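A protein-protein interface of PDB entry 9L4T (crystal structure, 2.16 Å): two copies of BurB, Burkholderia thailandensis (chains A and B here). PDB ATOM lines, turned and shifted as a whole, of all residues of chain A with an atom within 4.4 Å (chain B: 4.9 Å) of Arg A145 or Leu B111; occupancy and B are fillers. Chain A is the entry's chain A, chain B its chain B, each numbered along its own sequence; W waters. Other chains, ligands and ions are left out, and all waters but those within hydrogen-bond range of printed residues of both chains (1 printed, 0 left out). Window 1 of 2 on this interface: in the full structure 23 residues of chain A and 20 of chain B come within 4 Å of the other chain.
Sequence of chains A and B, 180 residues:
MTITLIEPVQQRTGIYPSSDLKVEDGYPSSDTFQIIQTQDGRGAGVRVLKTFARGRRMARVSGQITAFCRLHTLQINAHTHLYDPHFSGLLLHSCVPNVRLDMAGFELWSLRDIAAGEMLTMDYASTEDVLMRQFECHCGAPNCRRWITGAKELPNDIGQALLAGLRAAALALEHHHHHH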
ATOM      1  N   HIS A  93     -15.369  35.149  -5.789  1.00  0.00           N
ATOM      2  CA  HIS A  93     -14.389  34.128  -6.101  1.00  0.00           C
ATOM      3  C   HIS A  93     -14.915  33.151  -7.155  1.00  0.00           C
ATOM      4  O   HIS A  93     -16.123  32.905  -7.272  1.00  0.00           O
ATOM      5  CB  HIS A  93     -14.019  33.351  -4.837  1.00  0.00           C
ATOM      6  CG  HIS A  93     -13.341  32.045  -5.122  1.00  0.00           C
ATOM      7  ND1 HIS A  93     -11.983  31.951  -5.349  1.00  0.00           N
ATOM      8  CD2 HIS A  93     -13.838  30.791  -5.265  1.00  0.00           C
ATOM      9  CE1 HIS A  93     -11.670  30.690  -5.594  1.00  0.00           C
ATOM     10  NE2 HIS A  93     -12.778  29.969  -5.557  1.00  0.00           N
ATOM     11  N   CYS A  95     -13.266  29.230  -8.886  1.00  0.00           N
ATOM     12  CA  CYS A  95     -12.136  28.331  -9.091  1.00  0.00           C
ATOM     13  C   CYS A  95     -11.691  28.282 -10.548  1.00  0.00           C
ATOM     14  O   CYS A  95     -10.624  27.728 -10.830  1.00  0.00           O
ATOM     15  CB  CYS A  95     -12.483  26.916  -8.600  1.00  0.00           C
ATOM     16  SG  CYS A  95     -12.968  26.765  -6.839  1.00  0.00           S
ATOM     17  N   ASP A 123      -9.761  34.049  -8.609  1.00  0.00           N
ATOM     18  CA  ASP A 123      -9.364  33.042  -7.630  1.00  0.00           C
ATOM     19  C   ASP A 123      -8.747  33.750  -6.416  1.00  0.00           C
ATOM     20  O   ASP A 123      -7.599  34.216  -6.473  1.00  0.00           O
ATOM     21  CB  ASP A 123      -8.390  32.057  -8.271  1.00  0.00           C
ATOM     22  CG  ASP A 123      -8.003  30.907  -7.333  1.00  0.00           C
ATOM     23  OD1 ASP A 123      -8.425  30.933  -6.157  1.00  0.00           O
ATOM     24  OD2 ASP A 123      -7.276  29.974  -7.769  1.00  0.00           O
ATOM     25  N   ALA A 125      -7.409  32.636  -3.897  1.00  0.00           N
ATOM     26  CA  ALA A 125      -6.157  32.052  -3.452  1.00  0.00           C
ATOM     27  C   ALA A 125      -4.964  32.551  -4.261  1.00  0.00           C
ATOM     28  O   ALA A 125      -3.825  32.450  -3.786  1.00  0.00           O
ATOM     29  CB  ALA A 125      -6.232  30.532  -3.519  1.00  0.00           C
ATOM     30  N   ASN A 143     -13.645  21.142 -11.308  1.00  0.00           N
ATOM     31  CA  ASN A 143     -12.450  21.079 -10.484  1.00  0.00           C
ATOM     32  C   ASN A 143     -12.503  22.058  -9.319  1.00  0.00           C
ATOM     33  O   ASN A 143     -11.481  22.289  -8.664  1.00  0.00           O
ATOM     34  CB  ASN A 143     -11.216  21.323 -11.351  1.00  0.00           C
ATOM     35  CG  ASN A 143     -10.866  20.118 -12.225  1.00  0.00           C
ATOM     36  OD1 ASN A 143     -10.983  20.168 -13.457  1.00  0.00           O
ATOM     37  ND2 ASN A 143     -10.418  19.035 -11.589  1.00  0.00           N
ATOM     38  N   CYS A 144     -13.675  22.628  -9.053  1.00  0.00           N
ATOM     39  CA  CYS A 144     -13.887  23.512  -7.915  1.00  0.00           C
ATOM     40  C   CYS A 144     -13.474  22.857  -6.604  1.00  0.00           C
ATOM     41  O   CYS A 144     -13.883  21.732  -6.310  1.00  0.00           O
ATOM     42  CB  CYS A 144     -15.368  23.890  -7.862  1.00  0.00           C
ATOM     43  SG  CYS A 144     -15.960  24.598  -6.297  1.00  0.00           S
ATOM     44  N   ARG A 145     -12.676  23.577  -5.800  1.00  0.00           N
ATOM     45  CA  ARG A 145     -12.209  23.043  -4.514  1.00  0.00           C
ATOM     46  C   ARG A 145     -13.302  22.962  -3.454  1.00  0.00           C
ATOM     47  O   ARG A 145     -13.017  22.488  -2.346  1.00  0.00           O
ATOM     48  CB  ARG A 145     -11.068  23.879  -3.936  1.00  0.00           C
ATOM     49  CG  ARG A 145     -10.038  24.372  -4.915  1.00  0.00           C
ATOM     50  CD  ARG A 145      -9.041  25.289  -4.188  1.00  0.00           C
ATOM     51  NE  ARG A 145      -8.063  25.851  -5.111  1.00  0.00           N
ATOM     52  CZ  ARG A 145      -8.072  27.097  -5.561  1.00  0.00           C
ATOM     53  NH1 ARG A 145      -8.962  27.985  -5.138  1.00  0.00           N
ATOM     54  NH2 ARG A 145      -7.158  27.465  -6.452  1.00  0.00           N
ATOM     55  N   ARG A 146     -14.509  23.457  -3.743  1.00  0.00           N
ATOM     56  CA  ARG A 146     -15.692  23.341  -2.889  1.00  0.00           C
ATOM     57  C   ARG A 146     -15.578  24.174  -1.622  1.00  0.00           C
ATOM     58  O   ARG A 146     -16.564  24.773  -1.177  1.00  0.00           O
ATOM     59  CB  ARG A 146     -15.970  21.872  -2.519  1.00  0.00           C
ATOM     60  CG  ARG A 146     -15.992  20.938  -3.712  1.00  0.00           C
ATOM     61  CD  ARG A 146     -17.088  21.350  -4.655  1.00  0.00           C
ATOM     62  NE  ARG A 146     -18.388  21.218  -4.017  1.00  0.00           N
ATOM     63  CZ  ARG A 146     -19.309  20.337  -4.384  1.00  0.00           C
ATOM     64  NH1 ARG A 146     -19.096  19.486  -5.378  1.00  0.00           N
ATOM     65  NH2 ARG A 146     -20.472  20.312  -3.740  1.00  0.00           N
ATOM     66  N   TRP A 147     -14.398  24.201  -1.017  1.00  0.00           N
ATOM     67  CA  TRP A 147     -14.156  24.983   0.185  1.00  0.00           C
ATOM     68  C   TRP A 147     -12.988  25.924  -0.067  1.00  0.00           C
ATOM     69  O   TRP A 147     -11.924  25.482  -0.506  1.00  0.00           O
ATOM     70  CB  TRP A 147     -13.862  24.079   1.379  1.00  0.00           C
ATOM     71  CG  TRP A 147     -13.860  24.847   2.628  1.00  0.00           C
ATOM     72  CD1 TRP A 147     -12.768  25.317   3.305  1.00  0.00           C
ATOM     73  CD2 TRP A 147     -15.006  25.273   3.365  1.00  0.00           C
ATOM     74  NE1 TRP A 147     -13.167  26.012   4.425  1.00  0.00           N
ATOM     75  CE2 TRP A 147     -14.536  26.002   4.485  1.00  0.00           C
ATOM     76  CE3 TRP A 147     -16.386  25.115   3.190  1.00  0.00           C
ATOM     77  CZ2 TRP A 147     -15.401  26.555   5.433  1.00  0.00           C
ATOM     78  CZ3 TRP A 147     -17.245  25.673   4.127  1.00  0.00           C
ATOM     79  CH2 TRP A 147     -16.750  26.383   5.235  1.00  0.00           C
ATOM     80  N   LEU A 163     -15.634  19.025   3.469  1.00  0.00           N
ATOM     81  CA  LEU A 163     -14.701  18.306   2.605  1.00  0.00           C
ATOM     82  C   LEU A 163     -14.773  16.805   2.843  1.00  0.00           C
ATOM     83  O   LEU A 163     -14.595  16.017   1.907  1.00  0.00           O
ATOM     84  CB  LEU A 163     -13.274  18.816   2.834  1.00  0.00           C
ATOM     85  CG  LEU A 163     -12.911  20.164   2.186  1.00  0.00           C
ATOM     86  CD1 LEU A 163     -11.418  20.480   2.246  1.00  0.00           C
ATOM     87  CD2 LEU A 163     -13.391  20.195   0.750  1.00  0.00           C
ATOM     88  N   ARG B  54      -3.869  19.958   1.096  1.00  0.00           N
ATOM     89  CA  ARG B  54      -3.932  21.327   0.595  1.00  0.00           C
ATOM     90  C   ARG B  54      -3.596  22.321   1.707  1.00  0.00           C
ATOM     91  O   ARG B  54      -3.813  22.056   2.891  1.00  0.00           O
ATOM     92  CB  ARG B  54      -5.321  21.616   0.020  1.00  0.00           C
ATOM     93  CG  ARG B  54      -6.441  21.591   1.047  1.00  0.00           C
ATOM     94  CD  ARG B  54      -7.771  22.016   0.442  1.00  0.00           C
ATOM     95  NE  ARG B  54      -7.924  23.467   0.387  1.00  0.00           N
ATOM     96  CZ  ARG B  54      -9.068  24.075   0.111  1.00  0.00           C
ATOM     97  NH1 ARG B  54     -10.170  23.387  -0.138  1.00  0.00           N
ATOM     98  NH2 ARG B  54      -9.112  25.405   0.102  1.00  0.00           N
ATOM     99  N   PRO B  97      -4.458  23.933 -11.717  1.00  0.00           N
ATOM    100  CA  PRO B  97      -3.227  23.513 -11.041  1.00  0.00           C
ATOM    101  C   PRO B  97      -3.495  22.987  -9.636  1.00  0.00           C
ATOM    102  O   PRO B  97      -4.489  23.330  -8.986  1.00  0.00           O
ATOM    103  CB  PRO B  97      -2.398  24.801 -10.999  1.00  0.00           C
ATOM    104  CG  PRO B  97      -3.439  25.908 -10.972  1.00  0.00           C
ATOM    105  CD  PRO B  97      -4.586  25.398 -11.812  1.00  0.00           C
ATOM    106  N   ASN B  98      -2.580  22.144  -9.162  1.00  0.00           N
ATOM    107  CA  ASN B  98      -2.609  21.719  -7.768  1.00  0.00           C
ATOM    108  C   ASN B  98      -1.560  22.410  -6.887  1.00  0.00           C
ATOM    109  O   ASN B  98      -1.492  22.110  -5.688  1.00  0.00           O
ATOM    110  CB  ASN B  98      -2.447  20.197  -7.673  1.00  0.00           C
ATOM    111  CG  ASN B  98      -1.172  19.693  -8.330  1.00  0.00           C
ATOM    112  OD1 ASN B  98      -0.327  20.477  -8.780  1.00  0.00           O
ATOM    113  ND2 ASN B  98      -1.021  18.366  -8.373  1.00  0.00           N
ATOM    114  N   VAL B  99      -0.737  23.317  -7.444  1.00  0.00           N
ATOM    115  CA  VAL B  99       0.296  24.009  -6.679  1.00  0.00           C
ATOM    116  C   VAL B  99       0.301  25.478  -7.081  1.00  0.00           C
ATOM    117  O   VAL B  99      -0.032  25.834  -8.217  1.00  0.00           O
ATOM    118  CB  VAL B  99       1.719  23.413  -6.874  1.00  0.00           C
ATOM    119  CG1 VAL B  99       1.722  21.900  -6.741  1.00  0.00           C
ATOM    120  CG2 VAL B  99       2.386  23.882  -8.174  1.00  0.00           C
ATOM    121  N   ARG B 100       0.681  26.339  -6.138  1.00  0.00           N
ATOM    122  CA  ARG B 100       0.820  27.764  -6.403  1.00  0.00           C
ATOM    123  C   ARG B 100       2.238  28.201  -6.070  1.00  0.00           C
ATOM    124  O   ARG B 100       2.825  27.742  -5.085  1.00  0.00           O
ATOM    125  CB  ARG B 100      -0.178  28.622  -5.594  1.00  0.00           C
ATOM    126  CG  ARG B 100       0.100  30.107  -5.821  1.00  0.00           C
ATOM    127  CD  ARG B 100      -0.693  31.116  -4.985  1.00  0.00           C
ATOM    128  NE  ARG B 100       0.079  32.353  -4.981  1.00  0.00           N
ATOM    129  CZ  ARG B 100      -0.129  33.391  -4.185  1.00  0.00           C
ATOM    130  NH1 ARG B 100      -1.179  33.445  -3.377  1.00  0.00           N
ATOM    131  NH2 ARG B 100       0.742  34.405  -4.204  1.00  0.00           N
ATOM    132  N   TRP B 109       3.346  26.063  -2.612  1.00  0.00           N
ATOM    133  CA  TRP B 109       2.248  25.699  -1.716  1.00  0.00           C
ATOM    134  C   TRP B 109       1.217  24.844  -2.449  1.00  0.00           C
ATOM    135  O   TRP B 109       0.948  25.057  -3.644  1.00  0.00           O
ATOM    136  CB  TRP B 109       1.552  26.942  -1.125  1.00  0.00           C
ATOM    137  CG  TRP B 109       2.318  27.644  -0.034  1.00  0.00           C
ATOM    138  CD1 TRP B 109       3.419  28.458  -0.177  1.00  0.00           C
ATOM    139  CD2 TRP B 109       2.039  27.588   1.371  1.00  0.00           C
ATOM    140  NE1 TRP B 109       3.834  28.907   1.055  1.00  0.00           N
ATOM    141  CE2 TRP B 109       3.003  28.391   2.021  1.00  0.00           C
ATOM    142  CE3 TRP B 109       1.066  26.939   2.144  1.00  0.00           C
ATOM    143  CZ2 TRP B 109       3.018  28.561   3.413  1.00  0.00           C
ATOM    144  CZ3 TRP B 109       1.088  27.103   3.533  1.00  0.00           C
ATOM    145  CH2 TRP B 109       2.052  27.911   4.147  1.00  0.00           C
ATOM    146  N   SER B 110       0.650  23.869  -1.728  1.00  0.00           N
ATOM    147  CA  SER B 110      -0.381  22.992  -2.277  1.00  0.00           C
ATOM    148  C   SER B 110      -1.692  23.761  -2.348  1.00  0.00           C
ATOM    149  O   SER B 110      -2.161  24.278  -1.324  1.00  0.00           O
ATOM    150  CB  SER B 110      -0.553  21.749  -1.410  1.00  0.00           C
ATOM    151  OG  SER B 110      -0.592  22.100  -0.043  1.00  0.00           O
ATOM    152  N   LEU B 111      -2.272  23.856  -3.555  1.00  0.00           N
ATOM    153  CA  LEU B 111      -3.615  24.421  -3.699  1.00  0.00           C
ATOM    154  C   LEU B 111      -4.692  23.377  -3.439  1.00  0.00           C
ATOM    155  O   LEU B 111      -5.713  23.691  -2.815  1.00  0.00           O
ATOM    156  CB  LEU B 111      -3.816  25.017  -5.095  1.00  0.00           C
ATOM    157  CG  LEU B 111      -3.126  26.350  -5.407  1.00  0.00           C
ATOM    158  CD1 LEU B 111      -3.376  26.764  -6.873  1.00  0.00           C
ATOM    159  CD2 LEU B 111      -3.584  27.440  -4.426  1.00  0.00           C
ATOM    160  N   ARG B 112      -4.489  22.150  -3.939  1.00  0.00           N
ATOM    161  CA  ARG B 112      -5.379  21.004  -3.768  1.00  0.00           C
ATOM    162  C   ARG B 112      -4.736  19.975  -2.837  1.00  0.00           C
ATOM    163  O   ARG B 112      -3.571  20.099  -2.426  1.00  0.00           O
ATOM    164  CB  ARG B 112      -5.684  20.322  -5.114  1.00  0.00           C
ATOM    165  CG  ARG B 112      -5.962  21.226  -6.298  1.00  0.00           C
ATOM    166  CD  ARG B 112      -7.411  21.663  -6.340  1.00  0.00           C
ATOM    167  NE  ARG B 112      -8.008  21.584  -7.670  1.00  0.00           N
ATOM    168  CZ  ARG B 112      -8.156  22.625  -8.482  1.00  0.00           C
ATOM    169  NH1 ARG B 112      -7.669  23.822  -8.170  1.00  0.00           N
ATOM    170  NH2 ARG B 112      -8.799  22.463  -9.636  1.00  0.00           N
ATOM    171  N   ASP B 113      -5.511  18.938  -2.511  1.00  0.00           N
ATOM    172  CA  ASP B 113      -4.933  17.734  -1.944  1.00  0.00           C
ATOM    173  C   ASP B 113      -4.107  17.057  -3.024  1.00  0.00           C
ATOM    174  O   ASP B 113      -4.562  16.913  -4.168  1.00  0.00           O
ATOM    175  CB  ASP B 113      -6.024  16.782  -1.449  1.00  0.00           C
ATOM    176  CG  ASP B 113      -6.524  17.125  -0.059  1.00  0.00           C
ATOM    177  OD1 ASP B 113      -5.963  18.045   0.567  1.00  0.00           O
ATOM    178  OD2 ASP B 113      -7.501  16.481   0.397  1.00  0.00           O
HETATM  179  O   HOH W   1      -8.704  28.141  -1.826  1.00  0.00           O
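Of the 10 printed residues of chain B, 4 touch a printed residue of chain A. Hydrophobic or aromatic side chains of chain A that line the printed part of chain B: Leu A163. Among the printed residues, 7 pairs touch across the chains. Among the printed residues, no Asp or Glu carboxylate lies within 4 Å of a Lys or Arg side-chain nitrogen of the other chain.
Water W1 bridges the guanidinium group (NH1) of Arg A145 (3.3 Å) and the guanidinium group (NH2) of Arg B54 (3.4 Å).
No position is printed for both chains. Of the 7 pairs that touch across the chains among the printed residues, none has its exchanged pair printed and touching as well.
O of Ala A125 is in hydrogen-bond range of NH1 of Arg B100, at 2.9 Å. O of Asn A143 sits at hydrogen-bond distance from NH2 of Arg B112. O of Trp A147 lies within hydrogen-bond range of NH1 of Arg B54 (2.8 Å).
Among the printed residues, pairs that only touch across the chains: Arg A145 with Arg B54, Arg A145 with Leu B111, Arg A145 with Arg B112 and Leu A163 with Arg B54.
The backbone NH (N) of Arg A145 is in hydrogen-bond range of the side-chain sulfur (SG) of Cys A95, 3.4 Å away. The side-chain carboxylate (OD1) of Asp A123 sits at hydrogen-bond distance from the backbone NH (N) of Ala A125. The side-chain carboxylate (OD1) of Asp B113 lies within hydrogen-bond range of the backbone NH (N) of Arg B54 (2.9 Å). N of Leu B111 is in hydrogen-bond range of O of Asn B98 (2.9 Å). O of Asn B98 sits at hydrogen-bond distance from N of Arg B112, 3.5 Å away. O of Trp B109 sits at hydrogen-bond distance from N of Arg B100, 2.8 Å away.
Printed residues of chain B within 4 Å of Asn A143: Arg B112 (2.9 Å). Arg A145 touches just these residues of chain B: Arg B54, Leu B111 and Arg B112. Of the printed residues of chain B, Trp A147 touches Arg B54 (2.8 Å). Of the printed residues of chain B, Leu A163 touches Arg B54 (3.96 Å). Of the printed residues of chain A, Arg B100 touches Ala A125 (2.9 Å). Leu B111 touches one residue of chain A. Of the printed residues of chain A, Arg B112 touches Asn A143 (2.9 Å) and Arg A145 (3.7 Å). The nearest printed residue of chain A that does not touch Arg B100 is Arg A145 (7.1 Å).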
